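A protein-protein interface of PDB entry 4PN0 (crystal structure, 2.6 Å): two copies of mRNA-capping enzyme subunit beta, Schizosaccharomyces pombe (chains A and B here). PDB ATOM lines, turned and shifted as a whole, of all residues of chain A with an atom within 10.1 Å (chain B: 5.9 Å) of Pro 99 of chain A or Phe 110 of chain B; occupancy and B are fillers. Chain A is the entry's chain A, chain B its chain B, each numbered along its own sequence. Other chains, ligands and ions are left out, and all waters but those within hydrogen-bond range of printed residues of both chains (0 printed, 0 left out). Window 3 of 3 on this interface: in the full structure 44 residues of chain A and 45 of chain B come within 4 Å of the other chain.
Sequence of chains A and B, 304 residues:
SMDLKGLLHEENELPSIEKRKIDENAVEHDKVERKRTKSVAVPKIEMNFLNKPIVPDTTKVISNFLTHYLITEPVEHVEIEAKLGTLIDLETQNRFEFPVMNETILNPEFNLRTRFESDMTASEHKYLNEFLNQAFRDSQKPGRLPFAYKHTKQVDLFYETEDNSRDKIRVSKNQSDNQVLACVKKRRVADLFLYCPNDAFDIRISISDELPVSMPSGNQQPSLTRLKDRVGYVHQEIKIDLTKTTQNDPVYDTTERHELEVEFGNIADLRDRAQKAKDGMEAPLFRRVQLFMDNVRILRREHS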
ATOM      1  N   ASP A  89     -15.470   4.052  -0.125  1.00  0.00           N
ATOM      2  CA  ASP A  89     -15.946   3.041  -1.060  1.00  0.00           C
ATOM      3  C   ASP A  89     -16.100   3.697  -2.422  1.00  0.00           C
ATOM      4  O   ASP A  89     -16.892   4.627  -2.575  1.00  0.00           O
ATOM      5  CB  ASP A  89     -17.293   2.482  -0.598  1.00  0.00           C
ATOM      6  CG  ASP A  89     -17.687   1.211  -1.333  1.00  0.00           C
ATOM      7  OD1 ASP A  89     -17.280   1.030  -2.499  1.00  0.00           O
ATOM      8  OD2 ASP A  89     -18.415   0.390  -0.737  1.00  0.00           O
ATOM      9  N   PHE A  96     -16.790   4.134   3.561  1.00  0.00           N
ATOM     10  CA  PHE A  96     -17.050   2.703   3.508  1.00  0.00           C
ATOM     11  C   PHE A  96     -18.012   2.287   4.617  1.00  0.00           C
ATOM     12  O   PHE A  96     -17.876   2.717   5.762  1.00  0.00           O
ATOM     13  CB  PHE A  96     -15.728   1.941   3.632  1.00  0.00           C
ATOM     14  CG  PHE A  96     -15.838   0.466   3.366  1.00  0.00           C
ATOM     15  CD1 PHE A  96     -15.784  -0.023   2.072  1.00  0.00           C
ATOM     16  CD2 PHE A  96     -15.968  -0.431   4.414  1.00  0.00           C
ATOM     17  CE1 PHE A  96     -15.876  -1.381   1.825  1.00  0.00           C
ATOM     18  CE2 PHE A  96     -16.059  -1.790   4.173  1.00  0.00           C
ATOM     19  CZ  PHE A  96     -16.014  -2.266   2.878  1.00  0.00           C
ATOM     20  N   GLU A  97     -19.003   1.474   4.265  1.00  0.00           N
ATOM     21  CA  GLU A  97     -19.949   0.961   5.247  1.00  0.00           C
ATOM     22  C   GLU A  97     -19.901  -0.555   5.298  1.00  0.00           C
ATOM     23  O   GLU A  97     -19.846  -1.221   4.265  1.00  0.00           O
ATOM     24  CB  GLU A  97     -21.372   1.433   4.949  1.00  0.00           C
ATOM     25  CG  GLU A  97     -21.633   2.883   5.317  1.00  0.00           C
ATOM     26  CD  GLU A  97     -23.106   3.168   5.535  1.00  0.00           C
ATOM     27  OE1 GLU A  97     -23.850   2.224   5.873  1.00  0.00           O
ATOM     28  OE2 GLU A  97     -23.520   4.334   5.367  1.00  0.00           O
ATOM     29  N   PHE A  98     -19.920  -1.094   6.511  1.00  0.00           N
ATOM     30  CA  PHE A  98     -19.815  -2.529   6.713  1.00  0.00           C
ATOM     31  C   PHE A  98     -20.718  -2.957   7.861  1.00  0.00           C
ATOM     32  O   PHE A  98     -20.826  -2.254   8.865  1.00  0.00           O
ATOM     33  CB  PHE A  98     -18.367  -2.908   7.026  1.00  0.00           C
ATOM     34  CG  PHE A  98     -17.802  -3.961   6.118  1.00  0.00           C
ATOM     35  CD1 PHE A  98     -18.421  -4.270   4.918  1.00  0.00           C
ATOM     36  CD2 PHE A  98     -16.652  -4.651   6.471  1.00  0.00           C
ATOM     37  CE1 PHE A  98     -17.903  -5.244   4.086  1.00  0.00           C
ATOM     38  CE2 PHE A  98     -16.130  -5.623   5.643  1.00  0.00           C
ATOM     39  CZ  PHE A  98     -16.755  -5.922   4.449  1.00  0.00           C
ATOM     40  N   PRO A  99     -21.371  -4.121   7.718  1.00  0.00           N
ATOM     41  CA  PRO A  99     -22.241  -4.663   8.766  1.00  0.00           C
ATOM     42  C   PRO A  99     -21.434  -5.274   9.906  1.00  0.00           C
ATOM     43  O   PRO A  99     -21.737  -6.380  10.350  1.00  0.00           O
ATOM     44  CB  PRO A  99     -23.012  -5.760   8.032  1.00  0.00           C
ATOM     45  CG  PRO A  99     -22.072  -6.216   6.978  1.00  0.00           C
ATOM     46  CD  PRO A  99     -21.352  -4.981   6.523  1.00  0.00           C
ATOM     47  N   VAL A 100     -20.413  -4.559  10.366  1.00  0.00           N
ATOM     48  CA  VAL A 100     -19.569  -5.031  11.455  1.00  0.00           C
ATOM     49  C   VAL A 100     -19.578  -4.012  12.590  1.00  0.00           C
ATOM     50  O   VAL A 100     -19.838  -2.828  12.369  1.00  0.00           O
ATOM     51  CB  VAL A 100     -18.125  -5.281  10.982  1.00  0.00           C
ATOM     52  CG1 VAL A 100     -18.129  -6.141   9.729  1.00  0.00           C
ATOM     53  CG2 VAL A 100     -17.407  -3.964  10.718  1.00  0.00           C
ATOM     54  N   MET A 101     -19.298  -4.471  13.804  1.00  0.00           N
ATOM     55  CA  MET A 101     -19.432  -3.609  14.971  1.00  0.00           C
ATOM     56  C   MET A 101     -18.121  -3.366  15.712  1.00  0.00           C
ATOM     57  O   MET A 101     -18.124  -2.955  16.871  1.00  0.00           O
ATOM     58  CB  MET A 101     -20.493  -4.169  15.920  1.00  0.00           C
ATOM     59  CG  MET A 101     -21.865  -4.291  15.274  1.00  0.00           C
ATOM     60  SD  MET A 101     -23.213  -4.326  16.466  1.00  0.00           S
ATOM     61  CE  MET A 101     -22.814  -5.805  17.390  1.00  0.00           C
ATOM     62  N   ASN A 102     -17.004  -3.603  15.035  1.00  0.00           N
ATOM     63  CA  ASN A 102     -15.693  -3.421  15.646  1.00  0.00           C
ATOM     64  C   ASN A 102     -14.606  -3.144  14.615  1.00  0.00           C
ATOM     65  O   ASN A 102     -14.830  -3.274  13.409  1.00  0.00           O
ATOM     66  CB  ASN A 102     -15.322  -4.653  16.468  1.00  0.00           C
ATOM     67  CG  ASN A 102     -15.295  -5.913  15.635  1.00  0.00           C
ATOM     68  OD1 ASN A 102     -16.341  -6.470  15.302  1.00  0.00           O
ATOM     69  ND2 ASN A 102     -14.097  -6.370  15.286  1.00  0.00           N
ATOM     70  N   GLU A 103     -13.431  -2.757  15.105  1.00  0.00           N
ATOM     71  CA  GLU A 103     -12.268  -2.507  14.260  1.00  0.00           C
ATOM     72  C   GLU A 103     -11.990  -3.688  13.336  1.00  0.00           C
ATOM     73  O   GLU A 103     -11.749  -4.805  13.795  1.00  0.00           O
ATOM     74  CB  GLU A 103     -11.046  -2.220  15.135  1.00  0.00           C
ATOM     75  CG  GLU A 103      -9.740  -2.078  14.375  1.00  0.00           C
ATOM     76  CD  GLU A 103      -8.571  -1.780  15.293  1.00  0.00           C
ATOM     77  OE1 GLU A 103      -8.645  -0.792  16.057  1.00  0.00           O
ATOM     78  OE2 GLU A 103      -7.581  -2.542  15.258  1.00  0.00           O
ATOM     79  N   THR A 104     -12.028  -3.435  12.032  1.00  0.00           N
ATOM     80  CA  THR A 104     -11.923  -4.506  11.046  1.00  0.00           C
ATOM     81  C   THR A 104     -10.834  -4.275   9.999  1.00  0.00           C
ATOM     82  O   THR A 104     -10.857  -3.280   9.274  1.00  0.00           O
ATOM     83  CB  THR A 104     -13.263  -4.716  10.318  1.00  0.00           C
ATOM     84  OG1 THR A 104     -14.217  -5.283  11.223  1.00  0.00           O
ATOM     85  CG2 THR A 104     -13.084  -5.652   9.147  1.00  0.00           C
ATOM     86  N   LEU A 106      -9.323  -5.133   6.503  1.00  0.00           N
ATOM     87  CA  LEU A 106      -9.844  -5.638   5.240  1.00  0.00           C
ATOM     88  C   LEU A 106      -8.886  -6.596   4.539  1.00  0.00           C
ATOM     89  O   LEU A 106      -7.677  -6.556   4.761  1.00  0.00           O
ATOM     90  CB  LEU A 106     -10.161  -4.476   4.303  1.00  0.00           C
ATOM     91  CG  LEU A 106     -11.130  -3.429   4.846  1.00  0.00           C
ATOM     92  CD1 LEU A 106     -11.392  -2.370   3.797  1.00  0.00           C
ATOM     93  CD2 LEU A 106     -12.426  -4.090   5.286  1.00  0.00           C
ATOM     94  N   PHE A 110      -9.995  -5.630  -1.434  1.00  0.00           N
ATOM     95  CA  PHE A 110     -10.781  -4.417  -1.255  1.00  0.00           C
ATOM     96  C   PHE A 110      -9.986  -3.175  -1.636  1.00  0.00           C
ATOM     97  O   PHE A 110     -10.557  -2.173  -2.070  1.00  0.00           O
ATOM     98  CB  PHE A 110     -11.262  -4.301   0.193  1.00  0.00           C
ATOM     99  CG  PHE A 110     -12.715  -4.625   0.377  1.00  0.00           C
ATOM    100  CD1 PHE A 110     -13.591  -4.573  -0.695  1.00  0.00           C
ATOM    101  CD2 PHE A 110     -13.207  -4.974   1.621  1.00  0.00           C
ATOM    102  CE1 PHE A 110     -14.931  -4.866  -0.531  1.00  0.00           C
ATOM    103  CE2 PHE A 110     -14.549  -5.268   1.793  1.00  0.00           C
ATOM    104  CZ  PHE A 110     -15.411  -5.215   0.715  1.00  0.00           C
ATOM    105  N   TYR A 195     -11.068  -0.523   8.932  1.00  0.00           N
ATOM    106  CA  TYR A 195     -12.368   0.125   9.035  1.00  0.00           C
ATOM    107  C   TYR A 195     -12.805   0.208  10.494  1.00  0.00           C
ATOM    108  O   TYR A 195     -12.783  -0.789  11.218  1.00  0.00           O
ATOM    109  CB  TYR A 195     -13.406  -0.625   8.207  1.00  0.00           C
ATOM    110  CG  TYR A 195     -14.820  -0.143   8.419  1.00  0.00           C
ATOM    111  CD1 TYR A 195     -15.208   1.129   8.021  1.00  0.00           C
ATOM    112  CD2 TYR A 195     -15.771  -0.964   9.010  1.00  0.00           C
ATOM    113  CE1 TYR A 195     -16.502   1.572   8.215  1.00  0.00           C
ATOM    114  CE2 TYR A 195     -17.065  -0.532   9.205  1.00  0.00           C
ATOM    115  CZ  TYR A 195     -17.428   0.736   8.805  1.00  0.00           C
ATOM    116  OH  TYR A 195     -18.719   1.168   8.997  1.00  0.00           O
ATOM    117  N   PRO A 197     -15.975   1.443  12.454  1.00  0.00           N
ATOM    118  CA  PRO A 197     -17.376   1.884  12.421  1.00  0.00           C
ATOM    119  C   PRO A 197     -17.794   2.683  13.653  1.00  0.00           C
ATOM    120  O   PRO A 197     -18.788   3.409  13.600  1.00  0.00           O
ATOM    121  CB  PRO A 197     -18.153   0.566  12.369  1.00  0.00           C
ATOM    122  CG  PRO A 197     -17.245  -0.428  13.002  1.00  0.00           C
ATOM    123  CD  PRO A 197     -15.863  -0.019  12.583  1.00  0.00           C
ATOM    124  N   ASN A 198     -17.050   2.547  14.745  1.00  0.00           N
ATOM    125  CA  ASN A 198     -17.403   3.211  15.996  1.00  0.00           C
ATOM    126  C   ASN A 198     -16.738   4.572  16.156  1.00  0.00           C
ATOM    127  O   ASN A 198     -17.071   5.333  17.065  1.00  0.00           O
ATOM    128  CB  ASN A 198     -17.050   2.317  17.182  1.00  0.00           C
ATOM    129  CG  ASN A 198     -17.741   0.974  17.118  1.00  0.00           C
ATOM    130  OD1 ASN A 198     -18.891   0.876  16.689  1.00  0.00           O
ATOM    131  ND2 ASN A 198     -17.042  -0.074  17.540  1.00  0.00           N
ATOM    132  N   ASP B  89     -23.262 -19.380   5.826  1.00  0.00           N
ATOM    133  CA  ASP B  89     -23.955 -18.485   4.910  1.00  0.00           C
ATOM    134  C   ASP B  89     -25.136 -19.237   4.310  1.00  0.00           C
ATOM    135  O   ASP B  89     -24.956 -20.272   3.672  1.00  0.00           O
ATOM    136  CB  ASP B  89     -23.002 -18.028   3.803  1.00  0.00           C
ATOM    137  CG  ASP B  89     -23.539 -16.849   3.008  1.00  0.00           C
ATOM    138  OD1 ASP B  89     -24.756 -16.810   2.722  1.00  0.00           O
ATOM    139  OD2 ASP B  89     -22.734 -15.957   2.667  1.00  0.00           O
ATOM    140  N   PHE B  96     -19.377 -19.111   6.397  1.00  0.00           N
ATOM    141  CA  PHE B  96     -19.499 -17.707   6.037  1.00  0.00           C
ATOM    142  C   PHE B  96     -18.161 -17.152   5.563  1.00  0.00           C
ATOM    143  O   PHE B  96     -17.119 -17.427   6.159  1.00  0.00           O
ATOM    144  CB  PHE B  96     -20.009 -16.923   7.246  1.00  0.00           C
ATOM    145  CG  PHE B  96     -20.235 -15.467   6.979  1.00  0.00           C
ATOM    146  CD1 PHE B  96     -21.297 -15.048   6.195  1.00  0.00           C
ATOM    147  CD2 PHE B  96     -19.401 -14.513   7.536  1.00  0.00           C
ATOM    148  CE1 PHE B  96     -21.514 -13.705   5.956  1.00  0.00           C
ATOM    149  CE2 PHE B  96     -19.613 -13.166   7.303  1.00  0.00           C
ATOM    150  CZ  PHE B  96     -20.670 -12.762   6.512  1.00  0.00           C
ATOM    151  N   PHE B  98     -16.144 -13.615   4.572  1.00  0.00           N
ATOM    152  CA  PHE B  98     -16.135 -12.168   4.648  1.00  0.00           C
ATOM    153  C   PHE B  98     -14.705 -11.688   4.449  1.00  0.00           C
ATOM    154  O   PHE B  98     -13.768 -12.271   4.999  1.00  0.00           O
ATOM    155  CB  PHE B  98     -16.682 -11.711   6.001  1.00  0.00           C
ATOM    156  CG  PHE B  98     -17.544 -10.484   5.926  1.00  0.00           C
ATOM    157  CD1 PHE B  98     -18.533 -10.373   4.961  1.00  0.00           C
ATOM    158  CD2 PHE B  98     -17.381  -9.451   6.834  1.00  0.00           C
ATOM    159  CE1 PHE B  98     -19.331  -9.242   4.891  1.00  0.00           C
ATOM    160  CE2 PHE B  98     -18.176  -8.319   6.771  1.00  0.00           C
ATOM    161  CZ  PHE B  98     -19.152  -8.214   5.799  1.00  0.00           C
ATOM    162  N   ILE B 105     -17.294  -8.936  14.814  1.00  0.00           N
ATOM    163  CA  ILE B 105     -18.663  -9.030  15.304  1.00  0.00           C
ATOM    164  C   ILE B 105     -19.648  -8.495  14.271  1.00  0.00           C
ATOM    165  O   ILE B 105     -19.698  -7.293  14.010  1.00  0.00           O
ATOM    166  CB  ILE B 105     -18.858  -8.248  16.612  1.00  0.00           C
ATOM    167  CG1 ILE B 105     -17.896  -8.746  17.690  1.00  0.00           C
ATOM    168  CG2 ILE B 105     -20.291  -8.370  17.090  1.00  0.00           C
ATOM    169  CD1 ILE B 105     -18.006  -7.986  18.996  1.00  0.00           C
ATOM    170  N   LEU B 106     -20.434  -9.394  13.692  1.00  0.00           N
ATOM    171  CA  LEU B 106     -21.421  -9.013  12.691  1.00  0.00           C
ATOM    172  C   LEU B 106     -22.569  -8.237  13.318  1.00  0.00           C
ATOM    173  O   LEU B 106     -22.861  -8.388  14.502  1.00  0.00           O
ATOM    174  CB  LEU B 106     -21.976 -10.254  11.993  1.00  0.00           C
ATOM    175  CG  LEU B 106     -20.968 -11.141  11.267  1.00  0.00           C
ATOM    176  CD1 LEU B 106     -21.673 -12.335  10.653  1.00  0.00           C
ATOM    177  CD2 LEU B 106     -20.229 -10.345  10.205  1.00  0.00           C
ATOM    178  N   ASN B 107     -23.214  -7.405  12.510  1.00  0.00           N
ATOM    179  CA  ASN B 107     -24.432  -6.729  12.922  1.00  0.00           C
ATOM    180  C   ASN B 107     -25.588  -7.716  13.003  1.00  0.00           C
ATOM    181  O   ASN B 107     -25.657  -8.666  12.223  1.00  0.00           O
ATOM    182  CB  ASN B 107     -24.778  -5.593  11.957  1.00  0.00           C
ATOM    183  CG  ASN B 107     -24.319  -4.240  12.466  1.00  0.00           C
ATOM    184  OD1 ASN B 107     -23.412  -3.628  11.904  1.00  0.00           O
ATOM    185  ND2 ASN B 107     -24.950  -3.765  13.535  1.00  0.00           N
ATOM    186  N   PRO B 108     -26.501  -7.500  13.962  1.00  0.00           N
ATOM    187  CA  PRO B 108     -27.683  -8.345  14.151  1.00  0.00           C
ATOM    188  C   PRO B 108     -28.530  -8.478  12.888  1.00  0.00           C
ATOM    189  O   PRO B 108     -29.274  -9.451  12.756  1.00  0.00           O
ATOM    190  CB  PRO B 108     -28.466  -7.598  15.233  1.00  0.00           C
ATOM    191  CG  PRO B 108     -27.410  -6.943  16.038  1.00  0.00           C
ATOM    192  CD  PRO B 108     -26.358  -6.521  15.052  1.00  0.00           C
ATOM    193  N   GLU B 109     -28.411  -7.522  11.968  1.00  0.00           N
ATOM    194  CA  GLU B 109     -29.126  -7.587  10.694  1.00  0.00           C
ATOM    195  C   GLU B 109     -28.554  -8.656   9.764  1.00  0.00           C
ATOM    196  O   GLU B 109     -29.072  -8.877   8.669  1.00  0.00           O
ATOM    197  CB  GLU B 109     -29.123  -6.223   9.996  1.00  0.00           C
ATOM    198  CG  GLU B 109     -30.045  -5.184  10.626  1.00  0.00           C
ATOM    199  CD  GLU B 109     -29.492  -4.602  11.915  1.00  0.00           C
ATOM    200  OE1 GLU B 109     -28.308  -4.857  12.228  1.00  0.00           O
ATOM    201  OE2 GLU B 109     -30.242  -3.890  12.616  1.00  0.00           O
ATOM    202  N   PHE B 110     -27.483  -9.311  10.202  1.00  0.00           N
ATOM    203  CA  PHE B 110     -26.869 -10.385   9.433  1.00  0.00           C
ATOM    204  C   PHE B 110     -27.280 -11.743   9.994  1.00  0.00           C
ATOM    205  O   PHE B 110     -27.082 -12.777   9.355  1.00  0.00           O
ATOM    206  CB  PHE B 110     -25.345 -10.250   9.450  1.00  0.00           C
ATOM    207  CG  PHE B 110     -24.718 -10.331   8.093  1.00  0.00           C
ATOM    208  CD1 PHE B 110     -24.032  -9.251   7.567  1.00  0.00           C
ATOM    209  CD2 PHE B 110     -24.828 -11.485   7.335  1.00  0.00           C
ATOM    210  CE1 PHE B 110     -23.455  -9.325   6.313  1.00  0.00           C
ATOM    211  CE2 PHE B 110     -24.256 -11.565   6.080  1.00  0.00           C
ATOM    212  CZ  PHE B 110     -23.568 -10.483   5.569  1.00  0.00           C
ATOM    213  N   ASN B 111     -27.854 -11.728  11.193  1.00  0.00           N
ATOM    214  CA  ASN B 111     -28.324 -12.948  11.840  1.00  0.00           C
ATOM    215  C   ASN B 111     -29.427 -13.617  11.028  1.00  0.00           C
ATOM    216  O   ASN B 111     -29.562 -14.840  11.034  1.00  0.00           O
ATOM    217  CB  ASN B 111     -28.826 -12.649  13.255  1.00  0.00           C
ATOM    218  CG  ASN B 111     -27.753 -12.042  14.143  1.00  0.00           C
ATOM    219  OD1 ASN B 111     -26.755 -11.507  13.659  1.00  0.00           O
ATOM    220  ND2 ASN B 111     -27.958 -12.124  15.453  1.00  0.00           N
ATOM    221  N   LEU B 112     -30.203 -12.802  10.322  1.00  0.00           N
ATOM    222  CA  LEU B 112     -31.308 -13.291   9.506  1.00  0.00           C
ATOM    223  C   LEU B 112     -30.796 -13.931   8.216  1.00  0.00           C
ATOM    224  O   LEU B 112     -31.541 -14.615   7.512  1.00  0.00           O
ATOM    225  CB  LEU B 112     -32.262 -12.140   9.175  1.00  0.00           C
ATOM    226  CG  LEU B 112     -33.658 -12.489   8.656  1.00  0.00           C
ATOM    227  CD1 LEU B 112     -34.526 -13.056   9.774  1.00  0.00           C
ATOM    228  CD2 LEU B 112     -34.316 -11.274   8.018  1.00  0.00           C
ATOM    229  N   ARG B 113     -29.519 -13.713   7.917  1.00  0.00           N
ATOM    230  CA  ARG B 113     -28.935 -14.179   6.663  1.00  0.00           C
ATOM    231  C   ARG B 113     -27.916 -15.301   6.864  1.00  0.00           C
ATOM    232  O   ARG B 113     -27.405 -15.867   5.897  1.00  0.00           O
ATOM    233  CB  ARG B 113     -28.290 -13.009   5.919  1.00  0.00           C
ATOM    234  CG  ARG B 113     -29.204 -11.802   5.783  1.00  0.00           C
ATOM    235  CD  ARG B 113     -28.613 -10.744   4.866  1.00  0.00           C
ATOM    236  NE  ARG B 113     -29.488  -9.580   4.758  1.00  0.00           N
ATOM    237  CZ  ARG B 113     -29.316  -8.592   3.888  1.00  0.00           C
ATOM    238  NH1 ARG B 113     -28.299  -8.625   3.036  1.00  0.00           N
ATOM    239  NH2 ARG B 113     -30.163  -7.571   3.863  1.00  0.00           N
ATOM    240  N   THR B 114     -27.621 -15.618   8.120  1.00  0.00           N
ATOM    241  CA  THR B 114     -26.675 -16.683   8.429  1.00  0.00           C
ATOM    242  C   THR B 114     -27.264 -17.730   9.365  1.00  0.00           C
ATOM    243  O   THR B 114     -28.329 -17.538   9.954  1.00  0.00           O
ATOM    244  CB  THR B 114     -25.386 -16.141   9.075  1.00  0.00           C
ATOM    245  OG1 THR B 114     -25.708 -15.477  10.301  1.00  0.00           O
ATOM    246  CG2 THR B 114     -24.682 -15.173   8.143  1.00  0.00           C
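O of Pro 99 of chain A sits at hydrogen-bond distance from N of Asn 107 of chain B, at 2.8 Å. The backbone NH of Val 100 of chain A lies within hydrogen-bond range of the side-chain amide oxygen of Asn 107 of chain B (3.5 Å). N of Met 101 of chain A is in hydrogen-bond range of O of Ile 105 of chain B, at 2.9 Å. ND2 of Asn 107 of chain B lies within hydrogen-bond range of SD of Met 101 of chain A, 3.5 Å away. The side-chain amide oxygen (OD1) of Asn 102 of chain A lies within hydrogen-bond range of the backbone NH (N) of Ile 105 of chain B (2.7 Å).
O of Met 101 of chain A sits at hydrogen-bond distance from ND2 of Asn 198 of chain A (3.1 Å). The backbone carbonyl oxygen of Asn 102 of chain A is in hydrogen-bond range of the side-chain hydroxyl of Thr 104 of chain A, 3.0 Å away. The side-chain amide oxygen of Asn 111 of chain B lies close to the backbone carbonyl oxygen of Asn 107 of chain B, 3.4 Å away. The backbone carbonyl oxygen (O) of Phe 110 of chain B sits at hydrogen-bond distance from the side-chain hydroxyl (OG1) of Thr 114 of chain B, at 3.2 Å.
Among the printed residues, merely in contact across the chains: Val 100 of chain A with Ile 105 of chain B, Pro 99 of chain A with Phe 110 of chain B, Pro 99 of chain A with Leu 106 of chain B, Phe 98 of chain A with Phe 98 of chain B, Val 100 of chain A with Phe 98 of chain B, Pro 99 of chain A with Phe 98 of chain B and Met 101 of chain A with Leu 106 of chain B.
Pro 99 of chain A touches just these residues of chain B: Phe 98, Leu 106, Asn 107 and Phe 110. Phe 110 of chain B touches just one residue of chain A: Pro 99. No residue of chain A comes within 4 Å of Asn 111 of chain B. No residue of chain A comes within 4 Å of Thr 114 of chain B. Printed residues of chain B within 4 Å of Asn 102 of chain A: Ile 105 (2.7 Å). Of the printed residues of chain A, Ile 105 of chain B touches Val 100, Met 101 and Asn 102. Tyr 195 of chain A touches none of the printed residues of chain B.
Of the 15 printed residues of chain A, 5 touch a printed residue of chain B. Printed residues of chain A that touch a printed residue of chain B: Phe 98, Pro 99, Val 100, Met 101 and Asn 102. Hydrophobic or aromatic side chains of chain B within 4 Å of the printed part of chain A: Phe 98, Ile 105 and Phe 110. Along chain B the printed residues that touch a printed residue of chain A span positions 98 to 110.
Phe 98 of chain A touches its own counterpart, Phe 98 of chain B.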
